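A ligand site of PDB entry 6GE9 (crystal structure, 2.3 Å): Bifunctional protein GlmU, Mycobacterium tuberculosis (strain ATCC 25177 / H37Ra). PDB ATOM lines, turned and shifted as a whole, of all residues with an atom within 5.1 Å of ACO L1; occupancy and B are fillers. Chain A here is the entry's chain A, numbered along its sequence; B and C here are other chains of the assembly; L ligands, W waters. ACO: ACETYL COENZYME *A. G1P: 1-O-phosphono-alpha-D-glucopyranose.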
ATOM      1  N   HIS A 374     -29.540   3.699  -7.271  1.00  0.00           N
ATOM      2  CA  HIS A 374     -28.198   4.220  -7.026  1.00  0.00           C
ATOM      3  C   HIS A 374     -27.501   4.627  -8.317  1.00  0.00           C
ATOM      4  O   HIS A 374     -27.527   3.899  -9.313  1.00  0.00           O
ATOM      5  CB  HIS A 374     -27.324   3.194  -6.301  1.00  0.00           C
ATOM      6  CG  HIS A 374     -28.071   2.279  -5.393  1.00  0.00           C
ATOM      7  ND1 HIS A 374     -28.547   2.676  -4.153  1.00  0.00           N
ATOM      8  CD2 HIS A 374     -28.429   0.981  -5.522  1.00  0.00           C
ATOM      9  CE1 HIS A 374     -29.162   1.664  -3.571  1.00  0.00           C
ATOM     10  NE2 HIS A 374     -29.109   0.623  -4.379  1.00  0.00           N
ATOM     11  N   ASN A 388     -36.712  -2.587 -12.143  1.00  0.00           N
ATOM     12  CA  ASN A 388     -35.610  -2.265 -11.235  1.00  0.00           C
ATOM     13  C   ASN A 388     -34.354  -2.048 -12.065  1.00  0.00           C
ATOM     14  O   ASN A 388     -33.904  -2.964 -12.758  1.00  0.00           O
ATOM     15  CB  ASN A 388     -35.396  -3.362 -10.198  1.00  0.00           C
ATOM     16  CG  ASN A 388     -34.474  -2.941  -9.073  1.00  0.00           C
ATOM     17  OD1 ASN A 388     -34.925  -2.372  -8.077  1.00  0.00           O
ATOM     18  ND2 ASN A 388     -33.184  -3.219  -9.222  1.00  0.00           N
ATOM     19  N   ILE A 389     -33.791  -0.847 -11.996  1.00  0.00           N
ATOM     20  CA  ILE A 389     -32.598  -0.482 -12.741  1.00  0.00           C
ATOM     21  C   ILE A 389     -31.406  -0.608 -11.806  1.00  0.00           C
ATOM     22  O   ILE A 389     -31.366   0.018 -10.747  1.00  0.00           O
ATOM     23  CB  ILE A 389     -32.696   0.929 -13.324  1.00  0.00           C
ATOM     24  CG1 ILE A 389     -33.972   1.078 -14.164  1.00  0.00           C
ATOM     25  CG2 ILE A 389     -31.468   1.258 -14.155  1.00  0.00           C
ATOM     26  CD1 ILE A 389     -34.049   0.109 -15.321  1.00  0.00           C
ATOM     27  N   GLY A 390     -30.422  -1.421 -12.206  1.00  0.00           N
ATOM     28  CA  GLY A 390     -29.247  -1.616 -11.377  1.00  0.00           C
ATOM     29  C   GLY A 390     -28.438  -0.346 -11.218  1.00  0.00           C
ATOM     30  O   GLY A 390     -28.576   0.623 -11.979  1.00  0.00           O
ATOM     31  N   ALA A 391     -27.581  -0.353 -10.202  1.00  0.00           N
ATOM     32  CA  ALA A 391     -26.754   0.813  -9.907  1.00  0.00           C
ATOM     33  C   ALA A 391     -25.713   1.028 -10.992  1.00  0.00           C
ATOM     34  O   ALA A 391     -25.413   0.146 -11.801  1.00  0.00           O
ATOM     35  CB  ALA A 391     -26.067   0.646  -8.553  1.00  0.00           C
ATOM     36  N   THR A 414     -32.694  -4.964 -14.706  1.00  0.00           N
ATOM     37  CA  THR A 414     -31.432  -4.648 -15.356  1.00  0.00           C
ATOM     38  C   THR A 414     -30.294  -4.646 -14.341  1.00  0.00           C
ATOM     39  O   THR A 414     -30.439  -4.142 -13.228  1.00  0.00           O
ATOM     40  CB  THR A 414     -31.510  -3.293 -16.061  1.00  0.00           C
ATOM     41  OG1 THR A 414     -31.287  -2.249 -15.116  1.00  0.00           O
ATOM     42  CG2 THR A 414     -32.869  -3.115 -16.714  1.00  0.00           C
ATOM     43  N   GLY A 415     -29.165  -5.221 -14.740  1.00  0.00           N
ATOM     44  CA  GLY A 415     -28.038  -5.350 -13.836  1.00  0.00           C
ATOM     45  C   GLY A 415     -27.272  -4.057 -13.660  1.00  0.00           C
ATOM     46  O   GLY A 415     -27.487  -3.057 -14.348  1.00  0.00           O
ATOM     47  N   SER A 416     -26.350  -4.091 -12.709  1.00  0.00           N
ATOM     48  CA  SER A 416     -25.523  -2.926 -12.414  1.00  0.00           C
ATOM     49  C   SER A 416     -24.570  -2.641 -13.561  1.00  0.00           C
ATOM     50  O   SER A 416     -24.137  -3.544 -14.278  1.00  0.00           O
ATOM     51  CB  SER A 416     -24.745  -3.130 -11.117  1.00  0.00           C
ATOM     52  OG  SER A 416     -25.634  -3.291 -10.021  1.00  0.00           O
ATOM     53  N   THR A 432     -30.644  -8.113 -17.627  1.00  0.00           N
ATOM     54  CA  THR A 432     -29.322  -7.825 -18.165  1.00  0.00           C
ATOM     55  C   THR A 432     -28.303  -8.042 -17.059  1.00  0.00           C
ATOM     56  O   THR A 432     -28.520  -7.667 -15.909  1.00  0.00           O
ATOM     57  CB  THR A 432     -29.201  -6.387 -18.703  1.00  0.00           C
ATOM     58  OG1 THR A 432     -29.442  -5.449 -17.650  1.00  0.00           O
ATOM     59  CG2 THR A 432     -30.177  -6.145 -19.833  1.00  0.00           C
ATOM     60  N   GLY A 433     -27.181  -8.670 -17.416  1.00  0.00           N
ATOM     61  CA  GLY A 433     -26.138  -8.928 -16.446  1.00  0.00           C
ATOM     62  C   GLY A 433     -25.381  -7.672 -16.065  1.00  0.00           C
ATOM     63  O   GLY A 433     -25.509  -6.617 -16.695  1.00  0.00           O
ATOM     64  N   ALA A 434     -24.594  -7.790 -15.015  1.00  0.00           N
ATOM     65  CA  ALA A 434     -23.757  -6.686 -14.576  1.00  0.00           C
ATOM     66  C   ALA A 434     -22.683  -6.393 -15.606  1.00  0.00           C
ATOM     67  O   ALA A 434     -22.056  -7.301 -16.153  1.00  0.00           O
ATOM     68  CB  ALA A 434     -23.130  -6.988 -13.220  1.00  0.00           C
ATOM     69  N   LEU A 447     -32.014 -12.784 -21.308  1.00  0.00           N
ATOM     70  CA  LEU A 447     -30.908 -12.258 -20.513  1.00  0.00           C
ATOM     71  C   LEU A 447     -29.851 -11.726 -21.462  1.00  0.00           C
ATOM     72  O   LEU A 447     -29.382 -12.449 -22.344  1.00  0.00           O
ATOM     73  CB  LEU A 447     -30.325 -13.332 -19.597  1.00  0.00           C
ATOM     74  CG  LEU A 447     -28.920 -13.053 -19.061  1.00  0.00           C
ATOM     75  CD1 LEU A 447     -28.965 -11.964 -17.995  1.00  0.00           C
ATOM     76  CD2 LEU A 447     -28.288 -14.312 -18.490  1.00  0.00           C
ATOM     77  N   VAL A 449     -26.144 -10.143 -21.865  1.00  0.00           N
ATOM     78  CA  VAL A 449     -24.822  -9.971 -21.274  1.00  0.00           C
ATOM     79  C   VAL A 449     -23.850  -9.580 -22.392  1.00  0.00           C
ATOM     80  O   VAL A 449     -24.160  -9.681 -23.578  1.00  0.00           O
ATOM     81  CB  VAL A 449     -24.333 -11.241 -20.549  1.00  0.00           C
ATOM     82  CG1 VAL A 449     -25.281 -11.612 -19.426  1.00  0.00           C
ATOM     83  CG2 VAL A 449     -24.171 -12.390 -21.532  1.00  0.00           C
ATOM     84  N   SER A 450     -22.668  -9.129 -21.977  1.00  0.00           N
ATOM     85  CA  SER A 450     -21.655  -8.719 -22.932  1.00  0.00           C
ATOM     86  C   SER A 450     -20.262  -8.755 -22.319  1.00  0.00           C
ATOM     87  O   SER A 450     -19.257  -8.776 -23.038  1.00  0.00           O
ATOM     88  CB  SER A 450     -21.954  -7.321 -23.470  1.00  0.00           C
ATOM     89  OG  SER A 450     -21.892  -6.352 -22.434  1.00  0.00           O
ATOM     90  N   ALA A 451     -20.193  -8.764 -20.988  1.00  0.00           N
ATOM     91  CA  ALA A 451     -18.907  -8.776 -20.309  1.00  0.00           C
ATOM     92  C   ALA A 451     -18.195 -10.097 -20.513  1.00  0.00           C
ATOM     93  O   ALA A 451     -18.814 -11.166 -20.523  1.00  0.00           O
ATOM     94  CB  ALA A 451     -19.094  -8.494 -18.818  1.00  0.00           C
ATOM     95  N   GLY A 452     -16.870 -10.034 -20.678  1.00  0.00           N
ATOM     96  CA  GLY A 452     -16.064 -11.219 -20.833  1.00  0.00           C
ATOM     97  C   GLY A 452     -15.978 -12.009 -19.541  1.00  0.00           C
ATOM     98  O   GLY A 452     -16.335 -11.520 -18.467  1.00  0.00           O
ATOM     99  N   ARG B 455     -24.895 -10.600 -26.116  1.00  0.00           N
ATOM    100  CA  ARG B 455     -25.420 -11.943 -26.258  1.00  0.00           C
ATOM    101  C   ARG B 455     -26.769 -12.034 -25.562  1.00  0.00           C
ATOM    102  O   ARG B 455     -26.874 -11.712 -24.373  1.00  0.00           O
ATOM    103  CB  ARG B 455     -24.454 -12.991 -25.692  1.00  0.00           C
ATOM    104  CG  ARG B 455     -24.941 -14.416 -25.814  1.00  0.00           C
ATOM    105  CD  ARG B 455     -23.795 -15.410 -25.701  1.00  0.00           C
ATOM    106  NE  ARG B 455     -23.319 -15.543 -24.328  1.00  0.00           N
ATOM    107  CZ  ARG B 455     -23.645 -16.548 -23.510  1.00  0.00           C
ATOM    108  NH1 ARG B 455     -24.447 -17.510 -23.939  1.00  0.00           N
ATOM    109  NH2 ARG B 455     -23.161 -16.589 -22.279  1.00  0.00           N
ATOM    110  N   ILE B 457     -29.756 -14.407 -24.270  1.00  0.00           N
ATOM    111  CA  ILE B 457     -30.130 -15.755 -23.886  1.00  0.00           C
ATOM    112  C   ILE B 457     -31.641 -15.767 -23.711  1.00  0.00           C
ATOM    113  O   ILE B 457     -32.170 -15.339 -22.684  1.00  0.00           O
ATOM    114  CB  ILE B 457     -29.410 -16.199 -22.608  1.00  0.00           C
ATOM    115  CG1 ILE B 457     -27.902 -15.931 -22.731  1.00  0.00           C
ATOM    116  CG2 ILE B 457     -29.668 -17.667 -22.333  1.00  0.00           C
ATOM    117  CD1 ILE B 457     -27.133 -16.239 -21.477  1.00  0.00           C
ATOM    118  N   TRP B 460     -34.349 -16.987 -20.624  1.00  0.00           N
ATOM    119  CA  TRP B 460     -33.508 -17.293 -19.469  1.00  0.00           C
ATOM    120  C   TRP B 460     -34.242 -17.027 -18.168  1.00  0.00           C
ATOM    121  O   TRP B 460     -33.992 -17.714 -17.163  1.00  0.00           O
ATOM    122  CB  TRP B 460     -32.215 -16.488 -19.541  1.00  0.00           C
ATOM    123  CG  TRP B 460     -31.328 -16.623 -18.321  1.00  0.00           C
ATOM    124  CD1 TRP B 460     -30.280 -17.490 -18.163  1.00  0.00           C
ATOM    125  CD2 TRP B 460     -31.411 -15.881 -17.103  1.00  0.00           C
ATOM    126  NE1 TRP B 460     -29.713 -17.322 -16.928  1.00  0.00           N
ATOM    127  CE2 TRP B 460     -30.388 -16.346 -16.256  1.00  0.00           C
ATOM    128  CE3 TRP B 460     -32.256 -14.856 -16.642  1.00  0.00           C
ATOM    129  CZ2 TRP B 460     -30.181 -15.832 -14.978  1.00  0.00           C
ATOM    130  CZ3 TRP B 460     -32.049 -14.344 -15.377  1.00  0.00           C
ATOM    131  CH2 TRP B 460     -31.020 -14.826 -14.557  1.00  0.00           C
ATOM    132  N   LYS B 464     -34.326 -19.738 -15.054  1.00  0.00           N
ATOM    133  CA  LYS B 464     -33.555 -19.490 -13.846  1.00  0.00           C
ATOM    134  C   LYS B 464     -34.301 -18.650 -12.815  1.00  0.00           C
ATOM    135  O   LYS B 464     -33.869 -18.599 -11.654  1.00  0.00           O
ATOM    136  CB  LYS B 464     -32.226 -18.810 -14.193  1.00  0.00           C
ATOM    137  CG  LYS B 464     -31.404 -19.577 -15.224  1.00  0.00           C
ATOM    138  CD  LYS B 464     -31.100 -20.989 -14.749  1.00  0.00           C
ATOM    139  CE  LYS B 464     -30.161 -20.996 -13.559  1.00  0.00           C
ATOM    140  NZ  LYS B 464     -28.816 -20.452 -13.916  1.00  0.00           N
ATOM    141  N   ARG B 465     -35.384 -17.989 -13.204  1.00  0.00           N
ATOM    142  CA  ARG B 465     -36.264 -17.271 -12.274  1.00  0.00           C
ATOM    143  C   ARG B 465     -37.699 -17.733 -12.523  1.00  0.00           C
ATOM    144  O   ARG B 465     -38.539 -16.961 -13.006  1.00  0.00           O
ATOM    145  CB  ARG B 465     -36.132 -15.760 -12.451  1.00  0.00           C
ATOM    146  CG  ARG B 465     -34.728 -15.208 -12.244  1.00  0.00           C
ATOM    147  CD  ARG B 465     -34.305 -15.292 -10.794  1.00  0.00           C
ATOM    148  NE  ARG B 465     -33.071 -14.553 -10.553  1.00  0.00           N
ATOM    149  CZ  ARG B 465     -31.849 -15.070 -10.679  1.00  0.00           C
ATOM    150  NH1 ARG B 465     -30.783 -14.322 -10.436  1.00  0.00           N
ATOM    151  NH2 ARG B 465     -31.704 -16.333 -11.041  1.00  0.00           N
ATOM    152  N   TYR C 377     -21.484   2.230  -4.515  1.00  0.00           N
ATOM    153  CA  TYR C 377     -22.513   1.701  -3.637  1.00  0.00           C
ATOM    154  C   TYR C 377     -21.983   0.460  -2.943  1.00  0.00           C
ATOM    155  O   TYR C 377     -21.513  -0.471  -3.591  1.00  0.00           O
ATOM    156  CB  TYR C 377     -23.793   1.372  -4.413  1.00  0.00           C
ATOM    157  CG  TYR C 377     -24.773   0.532  -3.614  1.00  0.00           C
ATOM    158  CD1 TYR C 377     -25.573   1.121  -2.637  1.00  0.00           C
ATOM    159  CD2 TYR C 377     -24.898  -0.830  -3.828  1.00  0.00           C
ATOM    160  CE1 TYR C 377     -26.465   0.373  -1.905  1.00  0.00           C
ATOM    161  CE2 TYR C 377     -25.787  -1.583  -3.088  1.00  0.00           C
ATOM    162  CZ  TYR C 377     -26.571  -0.982  -2.133  1.00  0.00           C
ATOM    163  OH  TYR C 377     -27.460  -1.735  -1.393  1.00  0.00           O
ATOM    164  N   VAL C 394     -19.659  -1.167  -7.644  1.00  0.00           N
ATOM    165  CA  VAL C 394     -20.961  -1.524  -7.097  1.00  0.00           C
ATOM    166  C   VAL C 394     -20.863  -2.903  -6.453  1.00  0.00           C
ATOM    167  O   VAL C 394     -20.355  -3.844  -7.070  1.00  0.00           O
ATOM    168  CB  VAL C 394     -22.069  -1.521  -8.169  1.00  0.00           C
ATOM    169  CG1 VAL C 394     -23.322  -2.212  -7.654  1.00  0.00           C
ATOM    170  CG2 VAL C 394     -22.389  -0.094  -8.604  1.00  0.00           C
ATOM    171  N   PHE C 395     -21.343  -3.016  -5.209  1.00  0.00           N
ATOM    172  CA  PHE C 395     -21.459  -4.306  -4.533  1.00  0.00           C
ATOM    173  C   PHE C 395     -22.848  -4.848  -4.827  1.00  0.00           C
ATOM    174  O   PHE C 395     -23.824  -4.523  -4.148  1.00  0.00           O
ATOM    175  CB  PHE C 395     -21.204  -4.154  -3.041  1.00  0.00           C
ATOM    176  CG  PHE C 395     -19.758  -4.008  -2.686  1.00  0.00           C
ATOM    177  CD1 PHE C 395     -19.097  -2.802  -2.886  1.00  0.00           C
ATOM    178  CD2 PHE C 395     -19.042  -5.063  -2.154  1.00  0.00           C
ATOM    179  CE1 PHE C 395     -17.761  -2.654  -2.555  1.00  0.00           C
ATOM    180  CE2 PHE C 395     -17.701  -4.929  -1.822  1.00  0.00           C
ATOM    181  CZ  PHE C 395     -17.060  -3.725  -2.029  1.00  0.00           C
ATOM    182  N   VAL C 396     -22.947  -5.685  -5.860  1.00  0.00           N
ATOM    183  CA  VAL C 396     -24.223  -6.222  -6.315  1.00  0.00           C
ATOM    184  C   VAL C 396     -24.745  -7.188  -5.265  1.00  0.00           C
ATOM    185  O   VAL C 396     -24.215  -8.293  -5.096  1.00  0.00           O
ATOM    186  CB  VAL C 396     -24.098  -6.897  -7.677  1.00  0.00           C
ATOM    187  CG1 VAL C 396     -25.416  -7.533  -8.085  1.00  0.00           C
ATOM    188  CG2 VAL C 396     -23.638  -5.889  -8.727  1.00  0.00           C
ATOM    189  N   ASN C 397     -25.797  -6.789  -4.548  1.00  0.00           N
ATOM    190  CA  ASN C 397     -26.368  -7.593  -3.471  1.00  0.00           C
ATOM    191  C   ASN C 397     -27.818  -7.971  -3.746  1.00  0.00           C
ATOM    192  O   ASN C 397     -28.572  -8.251  -2.801  1.00  0.00           O
ATOM    193  CB  ASN C 397     -26.276  -6.842  -2.142  1.00  0.00           C
ATOM    194  CG  ASN C 397     -27.138  -5.590  -2.111  1.00  0.00           C
ATOM    195  OD1 ASN C 397     -27.383  -4.966  -3.136  1.00  0.00           O
ATOM    196  ND2 ASN C 397     -27.610  -5.230  -0.923  1.00  0.00           N
ATOM    197  N   TYR C 398     -28.234  -8.014  -5.007  1.00  0.00           N
ATOM    198  CA  TYR C 398     -29.623  -8.312  -5.348  1.00  0.00           C
ATOM    199  C   TYR C 398     -29.640  -8.988  -6.714  1.00  0.00           C
ATOM    200  O   TYR C 398     -29.426  -8.337  -7.737  1.00  0.00           O
ATOM    201  CB  TYR C 398     -30.472  -7.043  -5.348  1.00  0.00           C
ATOM    202  CG  TYR C 398     -31.947  -7.291  -5.612  1.00  0.00           C
ATOM    203  CD1 TYR C 398     -32.681  -8.142  -4.790  1.00  0.00           C
ATOM    204  CD2 TYR C 398     -32.595  -6.673  -6.668  1.00  0.00           C
ATOM    205  CE1 TYR C 398     -34.026  -8.359  -5.026  1.00  0.00           C
ATOM    206  CE2 TYR C 398     -33.941  -6.889  -6.904  1.00  0.00           C
ATOM    207  CZ  TYR C 398     -34.644  -7.736  -6.089  1.00  0.00           C
ATOM    208  OH  TYR C 398     -35.990  -7.952  -6.325  1.00  0.00           O
ATOM    209  N   ASP C 399     -29.900 -10.302  -6.724  1.00  0.00           N
ATOM    210  CA  ASP C 399     -29.968 -11.075  -7.950  1.00  0.00           C
ATOM    211  C   ASP C 399     -31.351 -11.063  -8.595  1.00  0.00           C
ATOM    212  O   ASP C 399     -31.583 -11.793  -9.561  1.00  0.00           O
ATOM    213  CB  ASP C 399     -29.525 -12.520  -7.695  1.00  0.00           C
ATOM    214  CG  ASP C 399     -30.366 -13.211  -6.626  1.00  0.00           C
ATOM    215  OD1 ASP C 399     -31.279 -12.570  -6.066  1.00  0.00           O
ATOM    216  OD2 ASP C 399     -30.115 -14.396  -6.354  1.00  0.00           O
ATOM    217  N   VAL C 421     -20.519  -9.245  -7.830  1.00  0.00           N
ATOM    218  CA  VAL C 421     -21.779  -9.987  -7.915  1.00  0.00           C
ATOM    219  C   VAL C 421     -21.795 -10.976  -6.763  1.00  0.00           C
ATOM    220  O   VAL C 421     -21.236 -12.068  -6.859  1.00  0.00           O
ATOM    221  CB  VAL C 421     -21.942 -10.680  -9.269  1.00  0.00           C
ATOM    222  CG1 VAL C 421     -23.339 -11.265  -9.400  1.00  0.00           C
ATOM    223  CG2 VAL C 421     -21.658  -9.702 -10.405  1.00  0.00           C
ATOM    224  N   VAL C 437     -15.995  -7.544 -13.858  1.00  0.00           N
ATOM    225  CA  VAL C 437     -17.217  -8.103 -13.288  1.00  0.00           C
ATOM    226  C   VAL C 437     -16.792  -9.348 -12.511  1.00  0.00           C
ATOM    227  O   VAL C 437     -16.507 -10.399 -13.091  1.00  0.00           O
ATOM    228  CB  VAL C 437     -18.253  -8.436 -14.364  1.00  0.00           C
ATOM    229  CG1 VAL C 437     -19.487  -9.063 -13.735  1.00  0.00           C
ATOM    230  CG2 VAL C 437     -18.626  -7.185 -15.140  1.00  0.00           C
ATOM    231  N   ARG C 439     -17.488 -12.375 -10.641  1.00  0.00           N
ATOM    232  CA  ARG C 439     -18.515 -13.370 -10.386  1.00  0.00           C
ATOM    233  C   ARG C 439     -17.999 -14.574  -9.612  1.00  0.00           C
ATOM    234  O   ARG C 439     -18.800 -15.372  -9.134  1.00  0.00           O
ATOM    235  CB  ARG C 439     -19.134 -13.848 -11.702  1.00  0.00           C
ATOM    236  CG  ARG C 439     -20.037 -12.826 -12.370  1.00  0.00           C
ATOM    237  CD  ARG C 439     -19.860 -12.841 -13.876  1.00  0.00           C
ATOM    238  NE  ARG C 439     -18.550 -12.318 -14.274  1.00  0.00           N
ATOM    239  CZ  ARG C 439     -18.100 -12.313 -15.519  1.00  0.00           C
ATOM    240  NH1 ARG C 439     -18.851 -12.787 -16.511  1.00  0.00           N
ATOM    241  NH2 ARG C 439     -16.894 -11.818 -15.787  1.00  0.00           N
HETATM  242  N1A ACO L   1     -21.550 -10.663 -17.275  1.00  0.00           N
HETATM  243  C2A ACO L   1     -21.292 -11.374 -18.393  1.00  0.00           C
HETATM  244  N3A ACO L   1     -21.769 -12.606 -18.612  1.00  0.00           N
HETATM  245  C4A ACO L   1     -22.562 -13.222 -17.710  1.00  0.00           C
HETATM  246  C5A ACO L   1     -22.893 -12.509 -16.465  1.00  0.00           C
HETATM  247  C6A ACO L   1     -22.331 -11.151 -16.288  1.00  0.00           C
HETATM  248  N6A ACO L   1     -22.586 -10.423 -15.172  1.00  0.00           N
HETATM  249  N7A ACO L   1     -23.687 -13.331 -15.742  1.00  0.00           N
HETATM  250  C8A ACO L   1     -23.849 -14.472 -16.471  1.00  0.00           C
HETATM  251  N9A ACO L   1     -23.171 -14.406 -17.625  1.00  0.00           N
HETATM  252  C1B ACO L   1     -23.138 -15.466 -18.667  1.00  0.00           C
HETATM  253  C2B ACO L   1     -22.529 -16.748 -18.130  1.00  0.00           C
HETATM  254  O2B ACO L   1     -21.194 -16.929 -18.604  1.00  0.00           O
HETATM  255  C3B ACO L   1     -23.439 -17.843 -18.650  1.00  0.00           C
HETATM  256  O3B ACO L   1     -22.983 -18.270 -19.930  1.00  0.00           O
HETATM  257  P3B ACO L   1     -22.426 -19.764 -20.200  1.00  0.00           P
HETATM  258  O7A ACO L   1     -22.683 -20.496 -18.903  1.00  0.00           O
HETATM  259  O8A ACO L   1     -20.976 -19.554 -20.546  1.00  0.00           O
HETATM  260  O9A ACO L   1     -23.282 -20.239 -21.359  1.00  0.00           O
HETATM  261  C4B ACO L   1     -24.769 -17.157 -18.864  1.00  0.00           C
HETATM  262  O4B ACO L   1     -24.494 -15.767 -19.021  1.00  0.00           O
HETATM  263  C5B ACO L   1     -25.712 -17.315 -17.684  1.00  0.00           C
HETATM  264  O5B ACO L   1     -25.723 -18.660 -17.219  1.00  0.00           O
HETATM  265  P1A ACO L   1     -25.925 -18.928 -15.647  1.00  0.00           P
HETATM  266  O1A ACO L   1     -24.565 -19.134 -15.026  1.00  0.00           O
HETATM  267  O2A ACO L   1     -27.005 -19.983 -15.478  1.00  0.00           O
HETATM  268  O3A ACO L   1     -26.521 -17.526 -15.137  1.00  0.00           O
HETATM  269  P2A ACO L   1     -26.645 -17.182 -13.573  1.00  0.00           P
HETATM  270  O4A ACO L   1     -27.878 -17.869 -13.037  1.00  0.00           O
HETATM  271  O5A ACO L   1     -25.309 -17.408 -12.907  1.00  0.00           O
HETATM  272  O6A ACO L   1     -26.923 -15.599 -13.600  1.00  0.00           O
HETATM  273  CBP ACO L   1     -26.620 -13.302 -12.942  1.00  0.00           C
HETATM  274  CCP ACO L   1     -26.294 -14.753 -12.639  1.00  0.00           C
HETATM  275  CDP ACO L   1     -27.940 -12.945 -12.276  1.00  0.00           C
HETATM  276  CEP ACO L   1     -26.738 -13.098 -14.450  1.00  0.00           C
HETATM  277  CAP ACO L   1     -25.472 -12.447 -12.390  1.00  0.00           C
HETATM  278  OAP ACO L   1     -24.254 -12.867 -13.014  1.00  0.00           O
HETATM  279  C9P ACO L   1     -25.670 -10.984 -12.627  1.00  0.00           C
HETATM  280  O9P ACO L   1     -25.220 -10.443 -13.629  1.00  0.00           O
HETATM  281  N8P ACO L   1     -26.331 -10.315 -11.692  1.00  0.00           N
HETATM  282  C7P ACO L   1     -26.479  -8.875 -11.710  1.00  0.00           C
HETATM  283  C6P ACO L   1     -27.694  -8.449 -10.893  1.00  0.00           C
HETATM  284  C5P ACO L   1     -27.647  -6.960 -10.641  1.00  0.00           C
HETATM  285  O5P ACO L   1     -26.680  -6.302 -10.981  1.00  0.00           O
HETATM  286  N4P ACO L   1     -28.711  -6.442 -10.026  1.00  0.00           N
HETATM  287  C3P ACO L   1     -29.109  -5.071 -10.234  1.00  0.00           C
HETATM  288  C2P ACO L   1     -29.406  -4.357  -8.925  1.00  0.00           C
HETATM  289  S1P ACO L   1     -28.197  -4.822  -7.738  1.00  0.00           S
HETATM  290  C   ACO L   1     -27.793  -3.324  -7.135  1.00  0.00           C
HETATM  291  O   ACO L   1     -28.465  -2.352  -7.461  1.00  0.00           O
HETATM  292  CH3 ACO L   1     -26.611  -3.207  -6.219  1.00  0.00           C
HETATM  293  C1  G1P L   2     -30.982  -3.323  -3.147  1.00  0.00           C
HETATM  294  C2  G1P L   2     -30.522  -3.108  -4.590  1.00  0.00           C
HETATM  295  C3  G1P L   2     -31.555  -2.292  -5.355  1.00  0.00           C
HETATM  296  C4  G1P L   2     -32.941  -2.909  -5.211  1.00  0.00           C
HETATM  297  C5  G1P L   2     -33.281  -3.145  -3.747  1.00  0.00           C
HETATM  298  C6  G1P L   2     -34.620  -3.868  -3.615  1.00  0.00           C
HETATM  299  O1  G1P L   2     -31.009  -2.057  -2.482  1.00  0.00           O
HETATM  300  O2  G1P L   2     -29.278  -2.409  -4.593  1.00  0.00           O
HETATM  301  O3  G1P L   2     -31.194  -2.246  -6.743  1.00  0.00           O
HETATM  302  O4  G1P L   2     -33.909  -2.028  -5.790  1.00  0.00           O
HETATM  303  O5  G1P L   2     -32.261  -3.942  -3.127  1.00  0.00           O
HETATM  304  O6  G1P L   2     -34.800  -4.274  -2.246  1.00  0.00           O
HETATM  305  P   G1P L   2     -30.883  -1.979  -0.883  1.00  0.00           P
HETATM  306  O1P G1P L   2     -30.136  -3.238  -0.502  1.00  0.00           O
HETATM  307  O2P G1P L   2     -30.097  -0.700  -0.647  1.00  0.00           O
HETATM  308  O3P G1P L   2     -32.308  -1.939  -0.399  1.00  0.00           O
HETATM  309  O   HOH W   1     -22.320  -8.542 -19.399  1.00  0.00           O
HETATM  310  O   HOH W   2     -26.601 -11.383  -8.959  1.00  0.00           O
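Water W1 lies within hydrogen-bond range of the backbone NH (N) of Ala 451, the backbone NH (N) of Ser 450, a nitrogen (N1A) of ACO L1 and the backbone carbonyl oxygen (O) of Ala 434.
Merely in contact with ACO L1: Ala 451, Gly 415, Gly 433, Arg 439 of chain C, Val 396 of chain C, Thr 414, Val 449, Ala 391, Trp 460 of chain B, Tyr 377 of chain C, Asn 397 of chain C, Ile 457 of chain B, Gly 390, Arg 465 of chain B, Val 437 of chain C, Phe 395 of chain C, Val 394 of chain C, His 374, Val 421 of chain C and Asn 388. 25 residues have an atom within 4 Å of ACO L1: His 374, Asn 388, Gly 390, Ala 391, Thr 414, Gly 415, Ser 416, Gly 433, Ala 434, Val 449, Ala 451, Arg 455 of chain B, Ile 457 of chain B, Trp 460 of chain B, Lys 464 of chain B, Arg 465 of chain B, Tyr 377 of chain C, Val 394 of chain C, Phe 395 of chain C, Val 396 of chain C, Asn 397 of chain C, Tyr 398 of chain C, Val 421 of chain C, Val 437 of chain C and Arg 439 of chain C.
The backbone NH (N) of Ser 416 is in hydrogen-bond range of an oxygen (O5P) of ACO L1 (2.8 Å). NE2 of His 374 is in hydrogen-bond range of O2 of G1P L2 (3.0 Å). The side-chain amide nitrogen of Asn 397 of chain C lies within hydrogen-bond range of an oxygen (O1P) of G1P L2, at 3.2 Å. The side-chain hydroxyl (OH) of Tyr 377 of chain C sits at hydrogen-bond distance from an oxygen (O2P) of G1P L2, at 2.9 Å. An oxygen (O4) of G1P L2 sits at hydrogen-bond distance from the side-chain amide oxygen (OD1) of Asn 388 (2.5 Å). An oxygen (O9A) of ACO L1 lies within salt-bridge range of the guanidinium group (NH2) of Arg 455 of chain B. The side-chain amino group (NZ) of Lys 464 of chain B is in salt-bridge range of an oxygen (O2A) of ACO L1 (2.4 Å). An oxygen (O9P) of ACO L1 is in hydrogen-bond range of the backbone NH (N) of Ala 434, at 3.1 Å. N4P of ACO L1 is in hydrogen-bond range of O of Tyr 398 of chain C (3.1 Å). OG of Ser 416 sits at hydrogen-bond distance from O5P of ACO L1, 3.3 Å away. A nitrogen (N6A) of ACO L1 is in hydrogen-bond range of the backbone carbonyl oxygen (O) of Ala 434 (3.3 Å).
The backbone NH (N) of Phe 395 of chain C sits at hydrogen-bond distance from the backbone carbonyl oxygen (O) of Tyr 377 of chain C, at 3.0 Å. The backbone carbonyl oxygen (O) of Val 449 sits at hydrogen-bond distance from the backbone NH (N) of Arg 455 of chain B, 2.8 Å away. The backbone NH (N) of Ile 457 of chain B is in hydrogen-bond range of the backbone carbonyl oxygen (O) of Leu 447, 2.8 Å away. O of Asn 388 is in hydrogen-bond range of N of Thr 414 (3.0 Å). O of Thr 414 sits at hydrogen-bond distance from N of Gly 390 (2.9 Å). O of Val 437 of chain C is in hydrogen-bond range of NE of Arg 439 of chain C, at 3.0 Å. The backbone NH (N) of Gly 415 sits at hydrogen-bond distance from the backbone carbonyl oxygen (O) of Thr 432 (2.8 Å). The guanidinium group (NH2) of Arg 439 of chain C is in hydrogen-bond range of the backbone carbonyl oxygen (O) of Gly 452.
O of ACO L1 is in hydrogen-bond range of O3 of G1P L2.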
